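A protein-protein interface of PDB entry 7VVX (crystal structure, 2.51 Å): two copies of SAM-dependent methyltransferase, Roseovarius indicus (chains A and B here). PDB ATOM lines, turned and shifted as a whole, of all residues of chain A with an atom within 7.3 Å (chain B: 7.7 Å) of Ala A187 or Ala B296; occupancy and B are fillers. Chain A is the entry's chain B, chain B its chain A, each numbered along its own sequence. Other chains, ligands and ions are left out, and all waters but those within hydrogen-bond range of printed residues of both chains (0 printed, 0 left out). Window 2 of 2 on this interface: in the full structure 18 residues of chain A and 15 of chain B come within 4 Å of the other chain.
Arg A183 touches Glu B212 (CB to O, 3.9 Å). Arg B186 touches Arg A186. CB of Ala A187 touches NH2 of Arg B186, at 3.9 Å. Ala B296 touches Ala A187 (CB to O, 3.7 Å).
Arg A186 touches its own counterpart, Arg B186. 3 positions are printed for both chains. Of the 5 pairs that touch across the chains among the printed residues, 1 has its exchanged pair printed and touching as well.
The side-chain hydroxyl (OH) of Tyr B216 sits at hydrogen-bond distance from the backbone NH (N) of Arg B186, 3.0 Å away. The side-chain hydroxyl (OG1) of Thr A188 lies within hydrogen-bond range of the backbone carbonyl oxygen (O) of Arg A184 (2.9 Å). N of Arg A186 sits at hydrogen-bond distance from OH of Tyr A216.
Of the printed residues of chain B, Arg A183 touches Glu B212. Ala A187 touches just these residues of chain B: Arg B186 (3.9 Å) and Ala B296 (3.7 Å). Printed residues of chain A within 4 Å of Arg B186: Arg A186 (3.99 Å) and Ala A187 (3.9 Å). Of chain A, only Ala A187 comes within 4 Å of Ala B296. The nearest printed residue of chain B that does not touch Arg A183 is Asn B214 (4.7 Å).
NE of Arg A184 lies within salt-bridge range of OE1 of Glu B212 (3.9 Å).
Printed residues of chain B that touch a printed residue of chain A: Arg B186, Glu B212 and Ala B296. Among the printed residues, 5 pairs touch across the chains. Among the printed residues, Asp or Glu carboxylates within 4 Å of a Lys or Arg side-chain nitrogen of the other chain: Arg A184 with Glu B212 (3.9 Å).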
ATOM      1  N   ILE A 103     -17.930 -24.169 -11.102  1.00  0.00           N
ATOM      2  CA  ILE A 103     -18.956 -24.737 -10.225  1.00  0.00           C
ATOM      3  C   ILE A 103     -20.363 -24.720 -10.816  1.00  0.00           C
ATOM      4  O   ILE A 103     -21.351 -24.749 -10.077  1.00  0.00           O
ATOM      5  CB  ILE A 103     -18.906 -23.989  -8.879  1.00  0.00           C
ATOM      6  CG1 ILE A 103     -19.418 -22.555  -9.008  1.00  0.00           C
ATOM      7  CG2 ILE A 103     -17.484 -23.969  -8.309  1.00  0.00           C
ATOM      8  CD1 ILE A 103     -19.465 -21.825  -7.672  1.00  0.00           C
ATOM      9  N   LEU A 181     -13.731 -17.789 -11.691  1.00  0.00           N
ATOM     10  CA  LEU A 181     -14.090 -18.568 -10.514  1.00  0.00           C
ATOM     11  C   LEU A 181     -14.468 -17.651  -9.362  1.00  0.00           C
ATOM     12  O   LEU A 181     -15.496 -17.863  -8.709  1.00  0.00           O
ATOM     13  CB  LEU A 181     -12.939 -19.490 -10.104  1.00  0.00           C
ATOM     14  CG  LEU A 181     -13.205 -20.167  -8.752  1.00  0.00           C
ATOM     15  CD1 LEU A 181     -14.519 -20.958  -8.801  1.00  0.00           C
ATOM     16  CD2 LEU A 181     -12.042 -21.060  -8.298  1.00  0.00           C
ATOM     17  N   LEU A 182     -13.646 -16.621  -9.100  1.00  0.00           N
ATOM     18  CA  LEU A 182     -13.920 -15.726  -7.972  1.00  0.00           C
ATOM     19  C   LEU A 182     -15.291 -15.066  -8.096  1.00  0.00           C
ATOM     20  O   LEU A 182     -15.994 -14.905  -7.095  1.00  0.00           O
ATOM     21  CB  LEU A 182     -12.835 -14.665  -7.852  1.00  0.00           C
ATOM     22  CG  LEU A 182     -11.420 -15.171  -7.553  1.00  0.00           C
ATOM     23  CD1 LEU A 182     -10.462 -14.001  -7.345  1.00  0.00           C
ATOM     24  CD2 LEU A 182     -11.422 -16.072  -6.331  1.00  0.00           C
ATOM     25  N   ARG A 183     -15.702 -14.690  -9.320  1.00  0.00           N
ATOM     26  CA  ARG A 183     -17.042 -14.133  -9.490  1.00  0.00           C
ATOM     27  C   ARG A 183     -18.106 -15.128  -9.051  1.00  0.00           C
ATOM     28  O   ARG A 183     -19.126 -14.739  -8.481  1.00  0.00           O
ATOM     29  CB  ARG A 183     -17.297 -13.727 -10.935  1.00  0.00           C
ATOM     30  CG  ARG A 183     -16.243 -12.859 -11.520  1.00  0.00           C
ATOM     31  CD  ARG A 183     -16.338 -11.466 -11.011  1.00  0.00           C
ATOM     32  NE  ARG A 183     -15.392 -10.613 -11.715  1.00  0.00           N
ATOM     33  CZ  ARG A 183     -15.664  -9.912 -12.816  1.00  0.00           C
ATOM     34  NH1 ARG A 183     -16.877  -9.930 -13.370  1.00  0.00           N
ATOM     35  NH2 ARG A 183     -14.710  -9.179 -13.368  1.00  0.00           N
ATOM     36  N   ARG A 184     -17.886 -16.419  -9.294  1.00  0.00           N
ATOM     37  CA  ARG A 184     -18.878 -17.402  -8.872  1.00  0.00           C
ATOM     38  C   ARG A 184     -18.887 -17.583  -7.354  1.00  0.00           C
ATOM     39  O   ARG A 184     -19.958 -17.617  -6.738  1.00  0.00           O
ATOM     40  CB  ARG A 184     -18.630 -18.729  -9.577  1.00  0.00           C
ATOM     41  CG  ARG A 184     -19.005 -18.704 -11.057  1.00  0.00           C
ATOM     42  CD  ARG A 184     -18.043 -19.576 -11.868  1.00  0.00           C
ATOM     43  NE  ARG A 184     -18.582 -19.948 -13.171  1.00  0.00           N
ATOM     44  CZ  ARG A 184     -18.515 -19.190 -14.259  1.00  0.00           C
ATOM     45  NH1 ARG A 184     -17.931 -18.001 -14.217  1.00  0.00           N
ATOM     46  NH2 ARG A 184     -19.045 -19.624 -15.392  1.00  0.00           N
ATOM     47  N   THR A 185     -17.707 -17.689  -6.722  1.00  0.00           N
ATOM     48  CA  THR A 185     -17.683 -17.988  -5.290  1.00  0.00           C
ATOM     49  C   THR A 185     -18.214 -16.815  -4.475  1.00  0.00           C
ATOM     50  O   THR A 185     -18.891 -17.021  -3.462  1.00  0.00           O
ATOM     51  CB  THR A 185     -16.270 -18.386  -4.834  1.00  0.00           C
ATOM     52  OG1 THR A 185     -15.362 -17.299  -5.035  1.00  0.00           O
ATOM     53  CG2 THR A 185     -15.775 -19.588  -5.602  1.00  0.00           C
ATOM     54  N   ARG A 186     -18.004 -15.623  -4.932  1.00  0.00           N
ATOM     55  CA  ARG A 186     -18.471 -14.496  -4.226  1.00  0.00           C
ATOM     56  C   ARG A 186     -19.933 -14.411  -4.172  1.00  0.00           C
ATOM     57  O   ARG A 186     -20.452 -13.917  -3.249  1.00  0.00           O
ATOM     58  CB  ARG A 186     -17.941 -13.267  -4.849  1.00  0.00           C
ATOM     59  CG  ARG A 186     -18.131 -12.038  -4.026  1.00  0.00           C
ATOM     60  CD  ARG A 186     -18.054 -10.828  -4.883  1.00  0.00           C
ATOM     61  NE  ARG A 186     -17.631  -9.708  -4.108  1.00  0.00           N
ATOM     62  CZ  ARG A 186     -18.190  -8.525  -4.192  1.00  0.00           C
ATOM     63  NH1 ARG A 186     -19.179  -8.347  -5.036  1.00  0.00           N
ATOM     64  NH2 ARG A 186     -17.786  -7.520  -3.444  1.00  0.00           N
ATOM     65  N   ALA A 187     -20.596 -14.893  -5.184  1.00  0.00           N
ATOM     66  CA  ALA A 187     -22.012 -14.890  -5.216  1.00  0.00           C
ATOM     67  C   ALA A 187     -22.579 -16.092  -4.570  1.00  0.00           C
ATOM     68  O   ALA A 187     -23.541 -16.000  -3.922  1.00  0.00           O
ATOM     69  CB  ALA A 187     -22.473 -14.844  -6.606  1.00  0.00           C
ATOM     70  N   THR A 188     -21.971 -17.230  -4.765  1.00  0.00           N
ATOM     71  CA  THR A 188     -22.458 -18.457  -4.223  1.00  0.00           C
ATOM     72  C   THR A 188     -22.130 -18.710  -2.796  1.00  0.00           C
ATOM     73  O   THR A 188     -22.892 -19.203  -2.095  1.00  0.00           O
ATOM     74  CB  THR A 188     -21.966 -19.598  -5.068  1.00  0.00           C
ATOM     75  OG1 THR A 188     -22.288 -19.322  -6.397  1.00  0.00           O
ATOM     76  CG2 THR A 188     -22.687 -20.718  -4.780  1.00  0.00           C
ATOM     77  N   ALA A 189     -20.972 -18.356  -2.373  1.00  0.00           N
ATOM     78  CA  ALA A 189     -20.548 -18.535  -0.983  1.00  0.00           C
ATOM     79  C   ALA A 189     -19.833 -17.272  -0.529  1.00  0.00           C
ATOM     80  O   ALA A 189     -18.605 -17.245  -0.386  1.00  0.00           O
ATOM     81  CB  ALA A 189     -19.647 -19.760  -0.829  1.00  0.00           C
ATOM     82  N   PRO A 190     -20.583 -16.192  -0.312  1.00  0.00           N
ATOM     83  CA  PRO A 190     -19.953 -14.906   0.044  1.00  0.00           C
ATOM     84  C   PRO A 190     -19.096 -14.942   1.288  1.00  0.00           C
ATOM     85  O   PRO A 190     -18.201 -14.097   1.420  1.00  0.00           O
ATOM     86  CB  PRO A 190     -21.156 -13.966   0.235  1.00  0.00           C
ATOM     87  CG  PRO A 190     -22.349 -14.880   0.411  1.00  0.00           C
ATOM     88  CD  PRO A 190     -22.042 -16.073  -0.475  1.00  0.00           C
ATOM     89  N   TYR A 216     -12.088  -9.752  -2.270  1.00  0.00           N
ATOM     90  CA  TYR A 216     -11.354 -10.625  -1.360  1.00  0.00           C
ATOM     91  C   TYR A 216     -10.087  -9.925  -0.894  1.00  0.00           C
ATOM     92  O   TYR A 216      -9.482  -9.150  -1.641  1.00  0.00           O
ATOM     93  CB  TYR A 216     -10.981 -11.990  -2.027  1.00  0.00           C
ATOM     94  CG  TYR A 216     -12.166 -12.878  -2.331  1.00  0.00           C
ATOM     95  CD1 TYR A 216     -12.665 -13.743  -1.374  1.00  0.00           C
ATOM     96  CD2 TYR A 216     -12.774 -12.870  -3.592  1.00  0.00           C
ATOM     97  CE1 TYR A 216     -13.741 -14.571  -1.645  1.00  0.00           C
ATOM     98  CE2 TYR A 216     -13.857 -13.685  -3.872  1.00  0.00           C
ATOM     99  CZ  TYR A 216     -14.338 -14.532  -2.894  1.00  0.00           C
ATOM    100  OH  TYR A 216     -15.428 -15.345  -3.143  1.00  0.00           O
ATOM    101  N   ARG B 186     -28.146  -6.134  -9.822  1.00  0.00           N
ATOM    102  CA  ARG B 186     -27.555  -6.800  -8.661  1.00  0.00           C
ATOM    103  C   ARG B 186     -27.385  -5.852  -7.471  1.00  0.00           C
ATOM    104  O   ARG B 186     -27.409  -6.287  -6.311  1.00  0.00           O
ATOM    105  CB  ARG B 186     -26.201  -7.398  -9.040  1.00  0.00           C
ATOM    106  CG  ARG B 186     -25.695  -8.384  -8.017  1.00  0.00           C
ATOM    107  CD  ARG B 186     -24.212  -8.370  -7.965  1.00  0.00           C
ATOM    108  NE  ARG B 186     -23.693  -9.538  -7.267  1.00  0.00           N
ATOM    109  CZ  ARG B 186     -22.430  -9.943  -7.343  1.00  0.00           C
ATOM    110  NH1 ARG B 186     -21.576  -9.259  -8.092  1.00  0.00           N
ATOM    111  NH2 ARG B 186     -22.025 -11.020  -6.673  1.00  0.00           N
ATOM    112  N   PRO B 190     -31.150  -7.145  -5.358  1.00  0.00           N
ATOM    113  CA  PRO B 190     -30.256  -8.317  -5.454  1.00  0.00           C
ATOM    114  C   PRO B 190     -30.956  -9.664  -5.457  1.00  0.00           C
ATOM    115  O   PRO B 190     -30.292 -10.685  -5.705  1.00  0.00           O
ATOM    116  CB  PRO B 190     -29.355  -8.174  -4.220  1.00  0.00           C
ATOM    117  CG  PRO B 190     -30.081  -7.214  -3.309  1.00  0.00           C
ATOM    118  CD  PRO B 190     -30.847  -6.290  -4.197  1.00  0.00           C
ATOM    119  N   ALA B 191     -32.254  -9.720  -5.190  1.00  0.00           N
ATOM    120  CA  ALA B 191     -32.977 -10.985  -5.197  1.00  0.00           C
ATOM    121  C   ALA B 191     -33.891 -11.144  -6.404  1.00  0.00           C
ATOM    122  O   ALA B 191     -34.536 -12.183  -6.540  1.00  0.00           O
ATOM    123  CB  ALA B 191     -33.797 -11.142  -3.911  1.00  0.00           C
ATOM    124  N   ALA B 192     -33.948 -10.157  -7.288  1.00  0.00           N
ATOM    125  CA  ALA B 192     -34.842 -10.195  -8.434  1.00  0.00           C
ATOM    126  C   ALA B 192     -34.265 -11.038  -9.569  1.00  0.00           C
ATOM    127  O   ALA B 192     -33.056 -11.057  -9.799  1.00  0.00           O
ATOM    128  CB  ALA B 192     -35.093  -8.773  -8.925  1.00  0.00           C
ATOM    129  N   PHE B 211     -23.746 -13.568 -17.489  1.00  0.00           N
ATOM    130  CA  PHE B 211     -24.504 -13.649 -16.245  1.00  0.00           C
ATOM    131  C   PHE B 211     -23.634 -14.115 -15.090  1.00  0.00           C
ATOM    132  O   PHE B 211     -23.665 -13.533 -14.000  1.00  0.00           O
ATOM    133  CB  PHE B 211     -25.691 -14.608 -16.408  1.00  0.00           C
ATOM    134  CG  PHE B 211     -26.834 -14.030 -17.196  1.00  0.00           C
ATOM    135  CD1 PHE B 211     -27.853 -13.334 -16.555  1.00  0.00           C
ATOM    136  CD2 PHE B 211     -26.875 -14.158 -18.583  1.00  0.00           C
ATOM    137  CE1 PHE B 211     -28.903 -12.791 -17.284  1.00  0.00           C
ATOM    138  CE2 PHE B 211     -27.922 -13.616 -19.317  1.00  0.00           C
ATOM    139  CZ  PHE B 211     -28.939 -12.936 -18.667  1.00  0.00           C
ATOM    140  N   GLU B 212     -22.883 -15.193 -15.310  1.00  0.00           N
ATOM    141  CA  GLU B 212     -22.009 -15.716 -14.273  1.00  0.00           C
ATOM    142  C   GLU B 212     -20.995 -14.670 -13.832  1.00  0.00           C
ATOM    143  O   GLU B 212     -20.650 -14.593 -12.649  1.00  0.00           O
ATOM    144  CB  GLU B 212     -21.297 -16.957 -14.790  1.00  0.00           C
ATOM    145  CG  GLU B 212     -22.216 -18.050 -15.200  1.00  0.00           C
ATOM    146  CD  GLU B 212     -22.559 -18.971 -14.050  1.00  0.00           C
ATOM    147  OE1 GLU B 212     -22.218 -18.640 -12.899  1.00  0.00           O
ATOM    148  OE2 GLU B 212     -23.156 -20.044 -14.308  1.00  0.00           O
ATOM    149  N   ASN B 214     -21.491 -11.729 -13.366  1.00  0.00           N
ATOM    150  CA  ASN B 214     -22.147 -10.614 -12.695  1.00  0.00           C
ATOM    151  C   ASN B 214     -23.144 -11.074 -11.650  1.00  0.00           C
ATOM    152  O   ASN B 214     -24.116 -10.386 -11.403  1.00  0.00           O
ATOM    153  CB  ASN B 214     -22.819  -9.692 -13.710  1.00  0.00           C
ATOM    154  CG  ASN B 214     -21.791  -8.930 -14.557  1.00  0.00           C
ATOM    155  OD1 ASN B 214     -21.105  -8.027 -14.054  1.00  0.00           O
ATOM    156  ND2 ASN B 214     -21.659  -9.307 -15.830  1.00  0.00           N
ATOM    157  N   GLY B 215     -22.933 -12.243 -11.047  1.00  0.00           N
ATOM    158  CA  GLY B 215     -23.678 -12.668  -9.875  1.00  0.00           C
ATOM    159  C   GLY B 215     -24.901 -13.529 -10.116  1.00  0.00           C
ATOM    160  O   GLY B 215     -25.562 -13.915  -9.139  1.00  0.00           O
ATOM    161  N   TYR B 216     -25.216 -13.863 -11.369  1.00  0.00           N
ATOM    162  CA  TYR B 216     -26.433 -14.581 -11.736  1.00  0.00           C
ATOM    163  C   TYR B 216     -26.080 -15.922 -12.371  1.00  0.00           C
ATOM    164  O   TYR B 216     -25.090 -16.020 -13.118  1.00  0.00           O
ATOM    165  CB  TYR B 216     -27.273 -13.793 -12.753  1.00  0.00           C
ATOM    166  CG  TYR B 216     -27.723 -12.434 -12.313  1.00  0.00           C
ATOM    167  CD1 TYR B 216     -28.936 -12.269 -11.642  1.00  0.00           C
ATOM    168  CD2 TYR B 216     -26.961 -11.311 -12.585  1.00  0.00           C
ATOM    169  CE1 TYR B 216     -29.371 -11.049 -11.250  1.00  0.00           C
ATOM    170  CE2 TYR B 216     -27.379 -10.062 -12.174  1.00  0.00           C
ATOM    171  CZ  TYR B 216     -28.587  -9.943 -11.499  1.00  0.00           C
ATOM    172  OH  TYR B 216     -29.024  -8.711 -11.093  1.00  0.00           O
ATOM    173  N   VAL B 217     -26.896 -16.940 -12.101  1.00  0.00           N
ATOM    174  CA  VAL B 217     -26.791 -18.231 -12.772  1.00  0.00           C
ATOM    175  C   VAL B 217     -27.837 -18.271 -13.882  1.00  0.00           C
ATOM    176  O   VAL B 217     -29.036 -18.136 -13.594  1.00  0.00           O
ATOM    177  CB  VAL B 217     -26.934 -19.417 -11.803  1.00  0.00           C
ATOM    178  CG1 VAL B 217     -28.070 -19.239 -10.894  1.00  0.00           C
ATOM    179  CG2 VAL B 217     -27.149 -20.707 -12.604  1.00  0.00           C
ATOM    180  N   GLY B 293     -31.511 -14.804 -15.622  1.00  0.00           N
ATOM    181  CA  GLY B 293     -30.456 -14.822 -14.632  1.00  0.00           C
ATOM    182  C   GLY B 293     -31.093 -14.812 -13.264  1.00  0.00           C
ATOM    183  O   GLY B 293     -31.865 -13.907 -12.938  1.00  0.00           O
ATOM    184  N   ARG B 294     -30.823 -15.832 -12.467  1.00  0.00           N
ATOM    185  CA  ARG B 294     -31.418 -15.929 -11.144  1.00  0.00           C
ATOM    186  C   ARG B 294     -30.309 -15.866 -10.110  1.00  0.00           C
ATOM    187  O   ARG B 294     -29.391 -16.701 -10.148  1.00  0.00           O
ATOM    188  CB  ARG B 294     -32.209 -17.225 -11.006  1.00  0.00           C
ATOM    189  CG  ARG B 294     -32.626 -17.553  -9.601  1.00  0.00           C
ATOM    190  CD  ARG B 294     -33.723 -18.613  -9.649  1.00  0.00           C
ATOM    191  NE  ARG B 294     -34.871 -18.145 -10.419  1.00  0.00           N
ATOM    192  CZ  ARG B 294     -35.836 -18.938 -10.867  1.00  0.00           C
ATOM    193  NH1 ARG B 294     -35.797 -20.238 -10.609  1.00  0.00           N
ATOM    194  NH2 ARG B 294     -36.845 -18.435 -11.569  1.00  0.00           N
ATOM    195  N   PRO B 295     -30.307 -14.929  -9.245  1.00  0.00           N
ATOM    196  CA  PRO B 295     -29.246 -14.817  -8.294  1.00  0.00           C
ATOM    197  C   PRO B 295     -29.264 -15.882  -7.299  1.00  0.00           C
ATOM    198  O   PRO B 295     -30.196 -16.552  -7.242  1.00  0.00           O
ATOM    199  CB  PRO B 295     -29.622 -13.583  -7.589  1.00  0.00           C
ATOM    200  CG  PRO B 295     -31.046 -13.632  -7.624  1.00  0.00           C
ATOM    201  CD  PRO B 295     -31.316 -13.938  -9.006  1.00  0.00           C
ATOM    202  N   ALA B 296     -28.231 -16.006  -6.505  1.00  0.00           N
ATOM    203  CA  ALA B 296     -28.148 -16.979  -5.446  1.00  0.00           C
ATOM    204  C   ALA B 296     -29.461 -17.186  -4.725  1.00  0.00           C
ATOM    205  O   ALA B 296     -29.688 -16.645  -3.664  1.00  0.00           O
ATOM    206  CB  ALA B 296     -27.116 -16.536  -4.452  1.00  0.00           C
